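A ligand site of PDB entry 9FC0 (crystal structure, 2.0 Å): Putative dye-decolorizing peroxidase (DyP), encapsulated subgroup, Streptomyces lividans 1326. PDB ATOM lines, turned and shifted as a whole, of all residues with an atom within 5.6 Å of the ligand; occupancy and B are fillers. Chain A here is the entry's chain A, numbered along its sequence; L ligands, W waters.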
ATOM      1  N   ASP A 146     -14.416  11.796 -21.712  1.00  0.00           N
ATOM      2  CA  ASP A 146     -14.938  10.721 -22.564  1.00  0.00           C
ATOM      3  C   ASP A 146     -16.459  10.706 -22.403  1.00  0.00           C
ATOM      4  O   ASP A 146     -17.045  11.531 -21.736  1.00  0.00           O
ATOM      5  CB  ASP A 146     -14.200   9.414 -22.296  1.00  0.00           C
ATOM      6  CG  ASP A 146     -14.334   8.896 -20.887  1.00  0.00           C
ATOM      7  OD1 ASP A 146     -15.375   9.207 -20.251  1.00  0.00           O
ATOM      8  OD2 ASP A 146     -13.384   8.211 -20.451  1.00  0.00           O
ATOM      9  N   LEU A 148     -18.322   8.744 -20.777  1.00  0.00           N
ATOM     10  CA  LEU A 148     -18.754   8.535 -19.382  1.00  0.00           C
ATOM     11  C   LEU A 148     -18.701   9.819 -18.529  1.00  0.00           C
ATOM     12  O   LEU A 148     -19.144   9.792 -17.380  1.00  0.00           O
ATOM     13  CB  LEU A 148     -17.908   7.433 -18.750  1.00  0.00           C
ATOM     14  CG  LEU A 148     -17.956   6.081 -19.474  1.00  0.00           C
ATOM     15  CD1 LEU A 148     -17.090   5.048 -18.763  1.00  0.00           C
ATOM     16  CD2 LEU A 148     -19.403   5.621 -19.631  1.00  0.00           C
ATOM     17  N   PHE A 150     -15.882  11.417 -17.606  1.00  0.00           N
ATOM     18  CA  PHE A 150     -14.599  11.501 -16.896  1.00  0.00           C
ATOM     19  C   PHE A 150     -13.501  12.006 -17.830  1.00  0.00           C
ATOM     20  O   PHE A 150     -13.488  11.702 -19.047  1.00  0.00           O
ATOM     21  CB  PHE A 150     -14.215  10.151 -16.297  1.00  0.00           C
ATOM     22  CG  PHE A 150     -14.985   9.838 -15.034  1.00  0.00           C
ATOM     23  CD1 PHE A 150     -16.361   9.562 -15.083  1.00  0.00           C
ATOM     24  CD2 PHE A 150     -14.371   9.898 -13.809  1.00  0.00           C
ATOM     25  CE1 PHE A 150     -17.073   9.316 -13.902  1.00  0.00           C
ATOM     26  CE2 PHE A 150     -15.089   9.662 -12.650  1.00  0.00           C
ATOM     27  CZ  PHE A 150     -16.425   9.364 -12.701  1.00  0.00           C
ATOM     28  N   VAL A 151     -12.551  12.743 -17.256  1.00  0.00           N
ATOM     29  CA  VAL A 151     -11.340  13.126 -17.990  1.00  0.00           C
ATOM     30  C   VAL A 151     -10.576  11.850 -18.342  1.00  0.00           C
ATOM     31  O   VAL A 151     -10.444  10.926 -17.525  1.00  0.00           O
ATOM     32  CB  VAL A 151     -10.459  14.085 -17.190  1.00  0.00           C
ATOM     33  CG1 VAL A 151      -9.179  14.459 -17.920  1.00  0.00           C
ATOM     34  CG2 VAL A 151     -11.229  15.344 -16.811  1.00  0.00           C
ATOM     35  N   ASP A 152     -10.030  11.841 -19.564  1.00  0.00           N
ATOM     36  CA  ASP A 152      -9.459  10.620 -20.139  1.00  0.00           C
ATOM     37  C   ASP A 152      -8.090  10.975 -20.740  1.00  0.00           C
ATOM     38  O   ASP A 152      -8.008  11.757 -21.712  1.00  0.00           O
ATOM     39  CB  ASP A 152     -10.494  10.045 -21.121  1.00  0.00           C
ATOM     40  CG  ASP A 152     -10.234   8.645 -21.586  1.00  0.00           C
ATOM     41  OD1 ASP A 152      -9.035   8.330 -21.789  1.00  0.00           O
ATOM     42  OD2 ASP A 152     -11.227   7.847 -21.749  1.00  0.00           O
ATOM     43  N   GLY A 153      -7.035  10.426 -20.166  1.00  0.00           N
ATOM     44  CA  GLY A 153      -5.655  10.607 -20.643  1.00  0.00           C
ATOM     45  C   GLY A 153      -4.670  11.099 -19.565  1.00  0.00           C
ATOM     46  O   GLY A 153      -3.454  11.162 -19.768  1.00  0.00           O
ATOM     47  N   THR A 154      -5.197  11.500 -18.406  1.00  0.00           N
ATOM     48  CA  THR A 154      -4.444  12.221 -17.398  1.00  0.00           C
ATOM     49  C   THR A 154      -3.139  11.528 -17.023  1.00  0.00           C
ATOM     50  O   THR A 154      -2.115  12.201 -16.950  1.00  0.00           O
ATOM     51  CB  THR A 154      -5.294  12.360 -16.142  1.00  0.00           C
ATOM     52  OG1 THR A 154      -6.593  12.822 -16.503  1.00  0.00           O
ATOM     53  CG2 THR A 154      -4.645  13.282 -15.127  1.00  0.00           C
ATOM     54  N   GLU A 155      -3.155  10.208 -16.745  1.00  0.00           N
ATOM     55  CA  GLU A 155      -1.967   9.548 -16.270  1.00  0.00           C
ATOM     56  C   GLU A 155      -1.116   8.965 -17.409  1.00  0.00           C
ATOM     57  O   GLU A 155      -0.214   8.174 -17.139  1.00  0.00           O
ATOM     58  CB  GLU A 155      -2.296   8.463 -15.237  1.00  0.00           C
ATOM     59  CG  GLU A 155      -2.675   9.008 -13.838  1.00  0.00           C
ATOM     60  CD  GLU A 155      -1.636   9.920 -13.196  1.00  0.00           C
ATOM     61  OE1 GLU A 155      -0.601   9.431 -12.965  1.00  0.00           O
ATOM     62  OE2 GLU A 155      -1.858  11.114 -13.011  1.00  0.00           O
ATOM     63  N   ASN A 156      -1.369   9.358 -18.671  1.00  0.00           N
ATOM     64  CA  ASN A 156      -0.432   8.976 -19.726  1.00  0.00           C
ATOM     65  C   ASN A 156       0.979   9.431 -19.365  1.00  0.00           C
ATOM     66  O   ASN A 156       1.157  10.560 -18.922  1.00  0.00           O
ATOM     67  CB  ASN A 156      -0.762   9.568 -21.077  1.00  0.00           C
ATOM     68  CG  ASN A 156      -1.692   8.701 -21.918  1.00  0.00           C
ATOM     69  OD1 ASN A 156      -1.633   7.481 -21.875  1.00  0.00           O
ATOM     70  ND2 ASN A 156      -2.604   9.318 -22.653  1.00  0.00           N
ATOM     71  N   GLN A 184      -9.549  -1.573 -29.435  1.00  0.00           N
ATOM     72  CA  GLN A 184     -10.861  -2.116 -29.151  1.00  0.00           C
ATOM     73  C   GLN A 184     -11.899  -0.987 -29.257  1.00  0.00           C
ATOM     74  O   GLN A 184     -11.756   0.055 -28.635  1.00  0.00           O
ATOM     75  CB  GLN A 184     -10.967  -2.691 -27.745  1.00  0.00           C
ATOM     76  CG  GLN A 184      -9.972  -3.802 -27.391  1.00  0.00           C
ATOM     77  CD  GLN A 184     -10.109  -4.177 -25.929  1.00  0.00           C
ATOM     78  OE1 GLN A 184      -9.802  -3.376 -25.019  1.00  0.00           O
ATOM     79  NE2 GLN A 184     -10.727  -5.333 -25.708  1.00  0.00           N
ATOM     80  N   TYR A 186     -15.387   0.215 -28.031  1.00  0.00           N
ATOM     81  CA  TYR A 186     -16.319  -0.029 -26.933  1.00  0.00           C
ATOM     82  C   TYR A 186     -17.595   0.792 -27.149  1.00  0.00           C
ATOM     83  O   TYR A 186     -17.505   1.961 -27.541  1.00  0.00           O
ATOM     84  CB  TYR A 186     -15.719   0.373 -25.594  1.00  0.00           C
ATOM     85  CG  TYR A 186     -14.678  -0.566 -24.986  1.00  0.00           C
ATOM     86  CD1 TYR A 186     -15.063  -1.623 -24.147  1.00  0.00           C
ATOM     87  CD2 TYR A 186     -13.309  -0.402 -25.221  1.00  0.00           C
ATOM     88  CE1 TYR A 186     -14.128  -2.499 -23.615  1.00  0.00           C
ATOM     89  CE2 TYR A 186     -12.382  -1.290 -24.706  1.00  0.00           C
ATOM     90  CZ  TYR A 186     -12.777  -2.319 -23.865  1.00  0.00           C
ATOM     91  OH  TYR A 186     -11.868  -3.219 -23.304  1.00  0.00           O
ATOM     92  N   HIS A 188     -21.025   2.002 -24.964  1.00  0.00           N
ATOM     93  CA  HIS A 188     -21.451   2.156 -23.572  1.00  0.00           C
ATOM     94  C   HIS A 188     -22.971   2.067 -23.442  1.00  0.00           C
ATOM     95  O   HIS A 188     -23.666   2.502 -24.299  1.00  0.00           O
ATOM     96  CB  HIS A 188     -20.932   3.467 -22.994  1.00  0.00           C
ATOM     97  CG  HIS A 188     -19.434   3.582 -22.995  1.00  0.00           C
ATOM     98  ND1 HIS A 188     -18.679   2.806 -22.156  1.00  0.00           N
ATOM     99  CD2 HIS A 188     -18.583   4.413 -23.707  1.00  0.00           C
ATOM    100  CE1 HIS A 188     -17.401   3.118 -22.417  1.00  0.00           C
ATOM    101  NE2 HIS A 188     -17.323   4.139 -23.308  1.00  0.00           N
ATOM    102  N   ILE A 205     -14.519   4.151 -11.579  1.00  0.00           N
ATOM    103  CA  ILE A 205     -13.346   4.620 -12.310  1.00  0.00           C
ATOM    104  C   ILE A 205     -12.113   4.606 -11.390  1.00  0.00           C
ATOM    105  O   ILE A 205     -11.040   4.142 -11.786  1.00  0.00           O
ATOM    106  CB  ILE A 205     -13.604   6.032 -12.914  1.00  0.00           C
ATOM    107  CG1 ILE A 205     -14.787   6.051 -13.882  1.00  0.00           C
ATOM    108  CG2 ILE A 205     -12.363   6.538 -13.613  1.00  0.00           C
ATOM    109  CD1 ILE A 205     -14.683   5.184 -15.067  1.00  0.00           C
ATOM    110  N   ARG A 207     -11.338   7.801  -9.621  1.00  0.00           N
ATOM    111  CA  ARG A 207     -10.952   9.203  -9.605  1.00  0.00           C
ATOM    112  C   ARG A 207     -12.225  10.029  -9.429  1.00  0.00           C
ATOM    113  O   ARG A 207     -13.317   9.555  -9.757  1.00  0.00           O
ATOM    114  CB  ARG A 207     -10.259   9.645 -10.916  1.00  0.00           C
ATOM    115  CG  ARG A 207      -9.086   8.749 -11.357  1.00  0.00           C
ATOM    116  CD  ARG A 207      -8.370   9.227 -12.616  1.00  0.00           C
ATOM    117  NE  ARG A 207      -7.615  10.448 -12.434  1.00  0.00           N
ATOM    118  CZ  ARG A 207      -6.370  10.510 -11.980  1.00  0.00           C
ATOM    119  NH1 ARG A 207      -5.618   9.428 -11.912  1.00  0.00           N
ATOM    120  NH2 ARG A 207      -5.844  11.683 -11.715  1.00  0.00           N
ATOM    121  N   ASP A 212     -10.914  15.328 -11.162  1.00  0.00           N
ATOM    122  CA  ASP A 212      -9.972  14.378 -11.745  1.00  0.00           C
ATOM    123  C   ASP A 212      -8.809  14.097 -10.792  1.00  0.00           C
ATOM    124  O   ASP A 212      -7.750  13.665 -11.216  1.00  0.00           O
ATOM    125  CB  ASP A 212      -9.406  14.882 -13.071  1.00  0.00           C
ATOM    126  CG  ASP A 212      -8.744  13.792 -13.903  1.00  0.00           C
ATOM    127  OD1 ASP A 212      -9.048  12.601 -13.689  1.00  0.00           O
ATOM    128  OD2 ASP A 212      -7.927  14.172 -14.766  1.00  0.00           O
ATOM    129  N   GLU A 214      -7.236  11.566  -8.149  1.00  0.00           N
ATOM    130  CA  GLU A 214      -7.275  10.147  -7.823  1.00  0.00           C
ATOM    131  C   GLU A 214      -7.804   9.923  -6.404  1.00  0.00           C
ATOM    132  O   GLU A 214      -7.477  10.682  -5.510  1.00  0.00           O
ATOM    133  CB  GLU A 214      -5.860   9.587  -7.932  1.00  0.00           C
ATOM    134  CG  GLU A 214      -5.785   8.079  -7.763  1.00  0.00           C
ATOM    135  CD  GLU A 214      -4.409   7.523  -8.111  1.00  0.00           C
ATOM    136  OE1 GLU A 214      -3.501   8.263  -8.412  1.00  0.00           O
ATOM    137  OE2 GLU A 214      -4.267   6.323  -8.072  1.00  0.00           O
ATOM    138  N   HIS A 225     -11.374   0.774 -12.210  1.00  0.00           N
ATOM    139  CA  HIS A 225     -10.593   0.810 -13.434  1.00  0.00           C
ATOM    140  C   HIS A 225      -9.130   1.148 -13.167  1.00  0.00           C
ATOM    141  O   HIS A 225      -8.229   0.474 -13.679  1.00  0.00           O
ATOM    142  CB  HIS A 225     -11.217   1.771 -14.451  1.00  0.00           C
ATOM    143  CG  HIS A 225     -10.574   1.717 -15.777  1.00  0.00           C
ATOM    144  ND1 HIS A 225     -10.397   0.555 -16.465  1.00  0.00           N
ATOM    145  CD2 HIS A 225     -10.043   2.739 -16.529  1.00  0.00           C
ATOM    146  CE1 HIS A 225      -9.788   0.865 -17.620  1.00  0.00           C
ATOM    147  NE2 HIS A 225      -9.642   2.213 -17.697  1.00  0.00           N
ATOM    148  N   VAL A 226      -8.905   2.166 -12.375  1.00  0.00           N
ATOM    149  CA  VAL A 226      -7.560   2.628 -12.105  1.00  0.00           C
ATOM    150  C   VAL A 226      -6.753   1.588 -11.283  1.00  0.00           C
ATOM    151  O   VAL A 226      -5.558   1.430 -11.481  1.00  0.00           O
ATOM    152  CB  VAL A 226      -7.539   4.010 -11.447  1.00  0.00           C
ATOM    153  CG1 VAL A 226      -6.170   4.339 -10.879  1.00  0.00           C
ATOM    154  CG2 VAL A 226      -7.952   5.076 -12.427  1.00  0.00           C
ATOM    155  N   THR A 229      -5.755  -1.366 -13.726  1.00  0.00           N
ATOM    156  CA  THR A 229      -4.869  -1.075 -14.842  1.00  0.00           C
ATOM    157  C   THR A 229      -3.546  -0.507 -14.353  1.00  0.00           C
ATOM    158  O   THR A 229      -2.735  -0.082 -15.175  1.00  0.00           O
ATOM    159  CB  THR A 229      -5.551  -0.186 -15.899  1.00  0.00           C
ATOM    160  OG1 THR A 229      -5.990   1.033 -15.330  1.00  0.00           O
ATOM    161  CG2 THR A 229      -6.744  -0.882 -16.526  1.00  0.00           C
ATOM    162  N   SER A 230      -3.368  -0.479 -13.022  1.00  0.00           N
ATOM    163  CA  SER A 230      -2.088  -0.119 -12.400  1.00  0.00           C
ATOM    164  C   SER A 230      -1.260  -1.387 -12.176  1.00  0.00           C
ATOM    165  O   SER A 230      -1.724  -2.268 -11.422  1.00  0.00           O
ATOM    166  CB  SER A 230      -2.284   0.575 -11.080  1.00  0.00           C
ATOM    167  OG  SER A 230      -2.878   1.824 -11.308  1.00  0.00           O
ATOM    168  N   ILE A 241       1.526   2.219 -20.492  1.00  0.00           N
ATOM    169  CA  ILE A 241       1.194   2.340 -21.897  1.00  0.00           C
ATOM    170  C   ILE A 241       0.803   3.780 -22.195  1.00  0.00           C
ATOM    171  O   ILE A 241       0.530   4.552 -21.291  1.00  0.00           O
ATOM    172  CB  ILE A 241       0.095   1.344 -22.263  1.00  0.00           C
ATOM    173  CG1 ILE A 241      -1.253   1.701 -21.654  1.00  0.00           C
ATOM    174  CG2 ILE A 241       0.516  -0.076 -21.899  1.00  0.00           C
ATOM    175  CD1 ILE A 241      -2.386   0.843 -22.146  1.00  0.00           C
ATOM    176  N   ARG A 243      -2.044   5.887 -24.272  1.00  0.00           N
ATOM    177  CA  ARG A 243      -3.412   5.773 -24.791  1.00  0.00           C
ATOM    178  C   ARG A 243      -3.813   7.051 -25.488  1.00  0.00           C
ATOM    179  O   ARG A 243      -3.326   8.128 -25.141  1.00  0.00           O
ATOM    180  CB  ARG A 243      -4.393   5.537 -23.642  1.00  0.00           C
ATOM    181  CG  ARG A 243      -4.172   4.223 -22.916  1.00  0.00           C
ATOM    182  CD  ARG A 243      -4.889   4.139 -21.607  1.00  0.00           C
ATOM    183  NE  ARG A 243      -4.313   5.067 -20.633  1.00  0.00           N
ATOM    184  CZ  ARG A 243      -4.940   6.115 -20.083  1.00  0.00           C
ATOM    185  NH1 ARG A 243      -6.273   6.255 -20.208  1.00  0.00           N
ATOM    186  NH2 ARG A 243      -4.252   6.961 -19.309  1.00  0.00           N
ATOM    187  N   ASN A 245      -7.506   7.490 -26.401  1.00  0.00           N
ATOM    188  CA  ASN A 245      -8.928   7.122 -26.499  1.00  0.00           C
ATOM    189  C   ASN A 245      -9.771   8.259 -27.083  1.00  0.00           C
ATOM    190  O   ASN A 245      -9.605   9.416 -26.740  1.00  0.00           O
ATOM    191  CB  ASN A 245      -9.485   6.748 -25.133  1.00  0.00           C
ATOM    192  CG  ASN A 245      -8.776   5.577 -24.490  1.00  0.00           C
ATOM    193  OD1 ASN A 245      -7.983   4.833 -25.102  1.00  0.00           O
ATOM    194  ND2 ASN A 245      -9.023   5.422 -23.215  1.00  0.00           N
ATOM    195  N   THR A 258     -16.432   4.686 -26.858  1.00  0.00           N
ATOM    196  CA  THR A 258     -15.023   5.032 -26.693  1.00  0.00           C
ATOM    197  C   THR A 258     -14.205   4.114 -27.613  1.00  0.00           C
ATOM    198  O   THR A 258     -14.273   2.893 -27.484  1.00  0.00           O
ATOM    199  CB  THR A 258     -14.529   4.817 -25.257  1.00  0.00           C
ATOM    200  OG1 THR A 258     -15.329   5.629 -24.406  1.00  0.00           O
ATOM    201  CG2 THR A 258     -13.063   5.158 -25.068  1.00  0.00           C
ATOM    202  N   PHE A 260     -10.752   2.735 -27.977  1.00  0.00           N
ATOM    203  CA  PHE A 260      -9.530   2.536 -27.220  1.00  0.00           C
ATOM    204  C   PHE A 260      -8.374   2.201 -28.179  1.00  0.00           C
ATOM    205  O   PHE A 260      -8.497   1.362 -29.046  1.00  0.00           O
ATOM    206  CB  PHE A 260      -9.680   1.377 -26.244  1.00  0.00           C
ATOM    207  CG  PHE A 260      -8.379   0.989 -25.584  1.00  0.00           C
ATOM    208  CD1 PHE A 260      -7.881   1.686 -24.516  1.00  0.00           C
ATOM    209  CD2 PHE A 260      -7.660  -0.102 -26.037  1.00  0.00           C
ATOM    210  CE1 PHE A 260      -6.665   1.334 -23.946  1.00  0.00           C
ATOM    211  CE2 PHE A 260      -6.456  -0.470 -25.456  1.00  0.00           C
ATOM    212  CZ  PHE A 260      -5.953   0.259 -24.412  1.00  0.00           C
ATOM    213  N   THR A 270       0.209  -4.485 -22.284  1.00  0.00           N
ATOM    214  CA  THR A 270      -1.190  -4.269 -22.593  1.00  0.00           C
ATOM    215  C   THR A 270      -2.052  -5.504 -22.281  1.00  0.00           C
ATOM    216  O   THR A 270      -3.173  -5.390 -21.757  1.00  0.00           O
ATOM    217  CB  THR A 270      -1.367  -3.818 -24.043  1.00  0.00           C
ATOM    218  OG1 THR A 270      -0.449  -2.768 -24.318  1.00  0.00           O
ATOM    219  CG2 THR A 270      -2.730  -3.213 -24.281  1.00  0.00           C
ATOM    220  N   MET A 273      -2.795  -5.990 -18.567  1.00  0.00           N
ATOM    221  CA  MET A 273      -3.878  -5.124 -18.128  1.00  0.00           C
ATOM    222  C   MET A 273      -5.237  -5.669 -18.577  1.00  0.00           C
ATOM    223  O   MET A 273      -6.192  -5.649 -17.804  1.00  0.00           O
ATOM    224  CB  MET A 273      -3.706  -3.706 -18.691  1.00  0.00           C
ATOM    225  CG  MET A 273      -2.554  -2.974 -18.110  1.00  0.00           C
ATOM    226  SD  MET A 273      -2.231  -1.411 -18.982  1.00  0.00           S
ATOM    227  CE  MET A 273      -0.819  -0.822 -18.062  1.00  0.00           C
ATOM    228  N   LEU A 274      -5.335  -6.156 -19.844  1.00  0.00           N
ATOM    229  CA  LEU A 274      -6.578  -6.721 -20.326  1.00  0.00           C
ATOM    230  C   LEU A 274      -6.993  -7.970 -19.545  1.00  0.00           C
ATOM    231  O   LEU A 274      -8.188  -8.151 -19.260  1.00  0.00           O
ATOM    232  CB  LEU A 274      -6.467  -7.040 -21.823  1.00  0.00           C
ATOM    233  CG  LEU A 274      -6.556  -5.831 -22.756  1.00  0.00           C
ATOM    234  CD1 LEU A 274      -6.180  -6.177 -24.145  1.00  0.00           C
ATOM    235  CD2 LEU A 274      -7.958  -5.240 -22.771  1.00  0.00           C
ATOM    236  N   MET A 277      -8.519  -6.900 -16.300  1.00  0.00           N
ATOM    237  CA  MET A 277      -9.835  -6.299 -16.465  1.00  0.00           C
ATOM    238  C   MET A 277     -10.929  -7.363 -16.702  1.00  0.00           C
ATOM    239  O   MET A 277     -12.032  -7.272 -16.170  1.00  0.00           O
ATOM    240  CB  MET A 277      -9.809  -5.316 -17.652  1.00  0.00           C
ATOM    241  CG  MET A 277      -9.022  -3.985 -17.386  1.00  0.00           C
ATOM    242  SD  MET A 277      -8.947  -2.993 -18.918  1.00  0.00           S
ATOM    243  CE  MET A 277     -10.676  -2.704 -19.240  1.00  0.00           C
ATOM    244  N   ILE A 289     -15.762  -1.072 -14.994  1.00  0.00           N
ATOM    245  CA  ILE A 289     -16.060  -0.287 -16.184  1.00  0.00           C
ATOM    246  C   ILE A 289     -16.730  -1.160 -17.240  1.00  0.00           C
ATOM    247  O   ILE A 289     -17.525  -0.680 -18.044  1.00  0.00           O
ATOM    248  CB  ILE A 289     -14.789   0.465 -16.702  1.00  0.00           C
ATOM    249  CG1 ILE A 289     -15.128   1.776 -17.391  1.00  0.00           C
ATOM    250  CG2 ILE A 289     -13.955  -0.393 -17.640  1.00  0.00           C
ATOM    251  CD1 ILE A 289     -13.934   2.616 -17.795  1.00  0.00           C
ATOM    252  N   LEU A 290     -16.462  -2.484 -17.202  1.00  0.00           N
ATOM    253  CA  LEU A 290     -17.016  -3.406 -18.179  1.00  0.00           C
ATOM    254  C   LEU A 290     -18.496  -3.698 -17.922  1.00  0.00           C
ATOM    255  O   LEU A 290     -19.191  -4.175 -18.845  1.00  0.00           O
ATOM    256  CB  LEU A 290     -16.194  -4.696 -18.219  1.00  0.00           C
ATOM    257  CG  LEU A 290     -14.758  -4.534 -18.673  1.00  0.00           C
ATOM    258  CD1 LEU A 290     -14.018  -5.865 -18.602  1.00  0.00           C
ATOM    259  CD2 LEU A 290     -14.661  -3.978 -20.091  1.00  0.00           C
ATOM    260  N   SER A 293     -19.775  -1.162 -20.439  1.00  0.00           N
ATOM    261  CA  SER A 293     -18.945  -1.046 -21.630  1.00  0.00           C
ATOM    262  C   SER A 293     -18.797  -2.428 -22.265  1.00  0.00           C
ATOM    263  O   SER A 293     -18.255  -3.329 -21.640  1.00  0.00           O
ATOM    264  CB  SER A 293     -17.569  -0.447 -21.323  1.00  0.00           C
ATOM    265  OG  SER A 293     -17.608   0.749 -20.541  1.00  0.00           O
HETATM  266  C1  LIG L   1      -7.139   5.224 -17.106  1.00  0.00           C
HETATM  267  C2  LIG L   1     -11.348   5.454 -19.318  1.00  0.00           C
HETATM  268  C3  LIG L   1     -10.314   1.173 -21.497  1.00  0.00           C
HETATM  269  C4  LIG L   1      -6.001   1.304 -19.554  1.00  0.00           C
HETATM  270  C5  LIG L   1      -8.401   5.648 -17.508  1.00  0.00           C
HETATM  271  C6  LIG L   1      -9.126   6.810 -16.946  1.00  0.00           C
HETATM  272  C7  LIG L   1     -10.288   6.825 -17.564  1.00  0.00           C
HETATM  273  C8  LIG L   1     -10.317   5.751 -18.503  1.00  0.00           C
HETATM  274  C9  LIG L   1     -11.416   7.803 -17.423  1.00  0.00           C
HETATM  275  C10 LIG L   1      -8.643   7.739 -15.844  1.00  0.00           C
HETATM  276  C11 LIG L   1      -7.785   8.944 -16.262  1.00  0.00           C
HETATM  277  C12 LIG L   1      -6.562   8.527 -17.045  1.00  0.00           C
HETATM  278  O1  LIG L   1      -6.759   8.279 -18.270  1.00  0.00           O
HETATM  279  O2  LIG L   1      -5.450   8.362 -16.470  1.00  0.00           O
HETATM  280  C13 LIG L   1     -11.429   4.309 -20.094  1.00  0.00           C
HETATM  281  C14 LIG L   1     -12.580   3.988 -20.868  1.00  0.00           C
HETATM  282  C15 LIG L   1     -12.328   2.799 -21.525  1.00  0.00           C
HETATM  283  C16 LIG L   1     -10.992   2.354 -21.083  1.00  0.00           C
HETATM  284  C17 LIG L   1     -13.873   4.792 -21.112  1.00  0.00           C
HETATM  285  C18 LIG L   1     -13.410   2.136 -22.316  1.00  0.00           C
HETATM  286  C19 LIG L   1     -13.590   0.848 -22.201  1.00  0.00           C
HETATM  287  C20 LIG L   1      -9.045   0.762 -21.193  1.00  0.00           C
HETATM  288  C21 LIG L   1      -8.291  -0.439 -21.581  1.00  0.00           C
HETATM  289  C22 LIG L   1      -7.052  -0.389 -20.977  1.00  0.00           C
HETATM  290  C23 LIG L   1      -7.061   0.869 -20.239  1.00  0.00           C
HETATM  291  C24 LIG L   1      -8.794  -1.528 -22.483  1.00  0.00           C
HETATM  292  C25 LIG L   1      -5.861  -1.250 -20.984  1.00  0.00           C
HETATM  293  C26 LIG L   1      -5.690  -2.292 -21.716  1.00  0.00           C
HETATM  294  C27 LIG L   1      -5.978   2.438 -18.739  1.00  0.00           C
HETATM  295  C28 LIG L   1      -4.788   2.805 -17.944  1.00  0.00           C
HETATM  296  C29 LIG L   1      -5.090   3.843 -17.214  1.00  0.00           C
HETATM  297  C30 LIG L   1      -6.488   4.102 -17.582  1.00  0.00           C
HETATM  298  C31 LIG L   1      -3.471   2.137 -17.867  1.00  0.00           C
HETATM  299  C32 LIG L   1      -4.234   4.674 -16.304  1.00  0.00           C
HETATM  300  C33 LIG L   1      -4.121   4.002 -14.958  1.00  0.00           C
HETATM  301  C34 LIG L   1      -3.136   4.737 -13.994  1.00  0.00           C
HETATM  302  O3  LIG L   1      -1.993   4.336 -13.957  1.00  0.00           O
HETATM  303  O4  LIG L   1      -3.457   5.701 -13.349  1.00  0.00           O
HETATM  304  N1  LIG L   1      -9.148   5.006 -18.411  1.00  0.00           N
HETATM  305  N2  LIG L   1     -10.585   3.311 -20.244  1.00  0.00           N
HETATM  306  N3  LIG L   1      -8.282   1.504 -20.354  1.00  0.00           N
HETATM  307  N4  LIG L   1      -6.967   3.263 -18.498  1.00  0.00           N
HETATM  308 FE1  LIG L   1      -8.719   3.280 -19.351  1.00  0.00          FE
HETATM  309  O   HOH W   1      -5.697   7.316 -14.013  1.00  0.00           O
HETATM  310  O   HOH W   2      -1.069   2.380 -15.469  1.00  0.00           O
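A ring nitrogen (NE2) of His 225 is bound to an iron atom (FE1) of the ligand (2.2 Å). An oxygen (O1) of the ligand lies within salt-bridge range of the guanidinium group of Arg 243 (2.8 Å). The backbone NH of Gly 153 lies within hydrogen-bond range of an oxygen (O1) of the ligand (2.9 Å). N of Glu 155 lies within hydrogen-bond range of O2 of the ligand, 3.0 Å away.
The backbone NH (N) of His 225 is in hydrogen-bond range of the backbone carbonyl oxygen (O) of Ile 205, 3.4 Å away. OD1 of Asp 152 is in salt-bridge range of NH1 of Arg 243. O of Arg 243 sits at hydrogen-bond distance from ND2 of Asn 156 (2.9 Å). The backbone carbonyl oxygen of Gln 184 lies within hydrogen-bond range of the backbone NH of Phe 260, 2.9 Å away. OD1 of Asp 152 is in hydrogen-bond range of ND2 of Asn 245 (3.2 Å). OD1 of Asp 212 is in salt-bridge range of NE of Arg 207, 2.9 Å away. OG of Ser 230 sits at hydrogen-bond distance from O of Val 226, at 2.7 Å. N of Val 226 lies within hydrogen-bond range of O of Ile 205, at 3.0 Å.
Residues that only touch the ligand: Val 151, Tyr 186, Gln 184, Phe 260, Thr 229, Asp 152, Asp 146, Thr 154, Arg 207, Ile 289, Thr 258, Met 277, Ser 230, Leu 274, Phe 150, Met 273, Val 226, Asn 245, Leu 148 and Thr 270. Hydrophobic or aromatic side chains that line the ligand: Leu 148, Phe 150, Tyr 186, His 225, Val 226, Phe 260, Met 273, Leu 274, Met 277 and Ile 289. Of the 32 residues printed, 24 come within 4 Å of the ligand. Along chain A the residues within 4 Å of the ligand span positions 146 to 289. The nearest printed residue that does not touch the ligand is His 188 (4.1 Å).
Water W2 lies within hydrogen-bond range of an oxygen (O3) of the ligand (2.6 Å) and the backbone carbonyl oxygen (O) of Thr 229 (3.0 Å). Water W1 lies within hydrogen-bond range of an oxygen (O2) of the ligand and the guanidinium group (NH1) of Arg 207.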
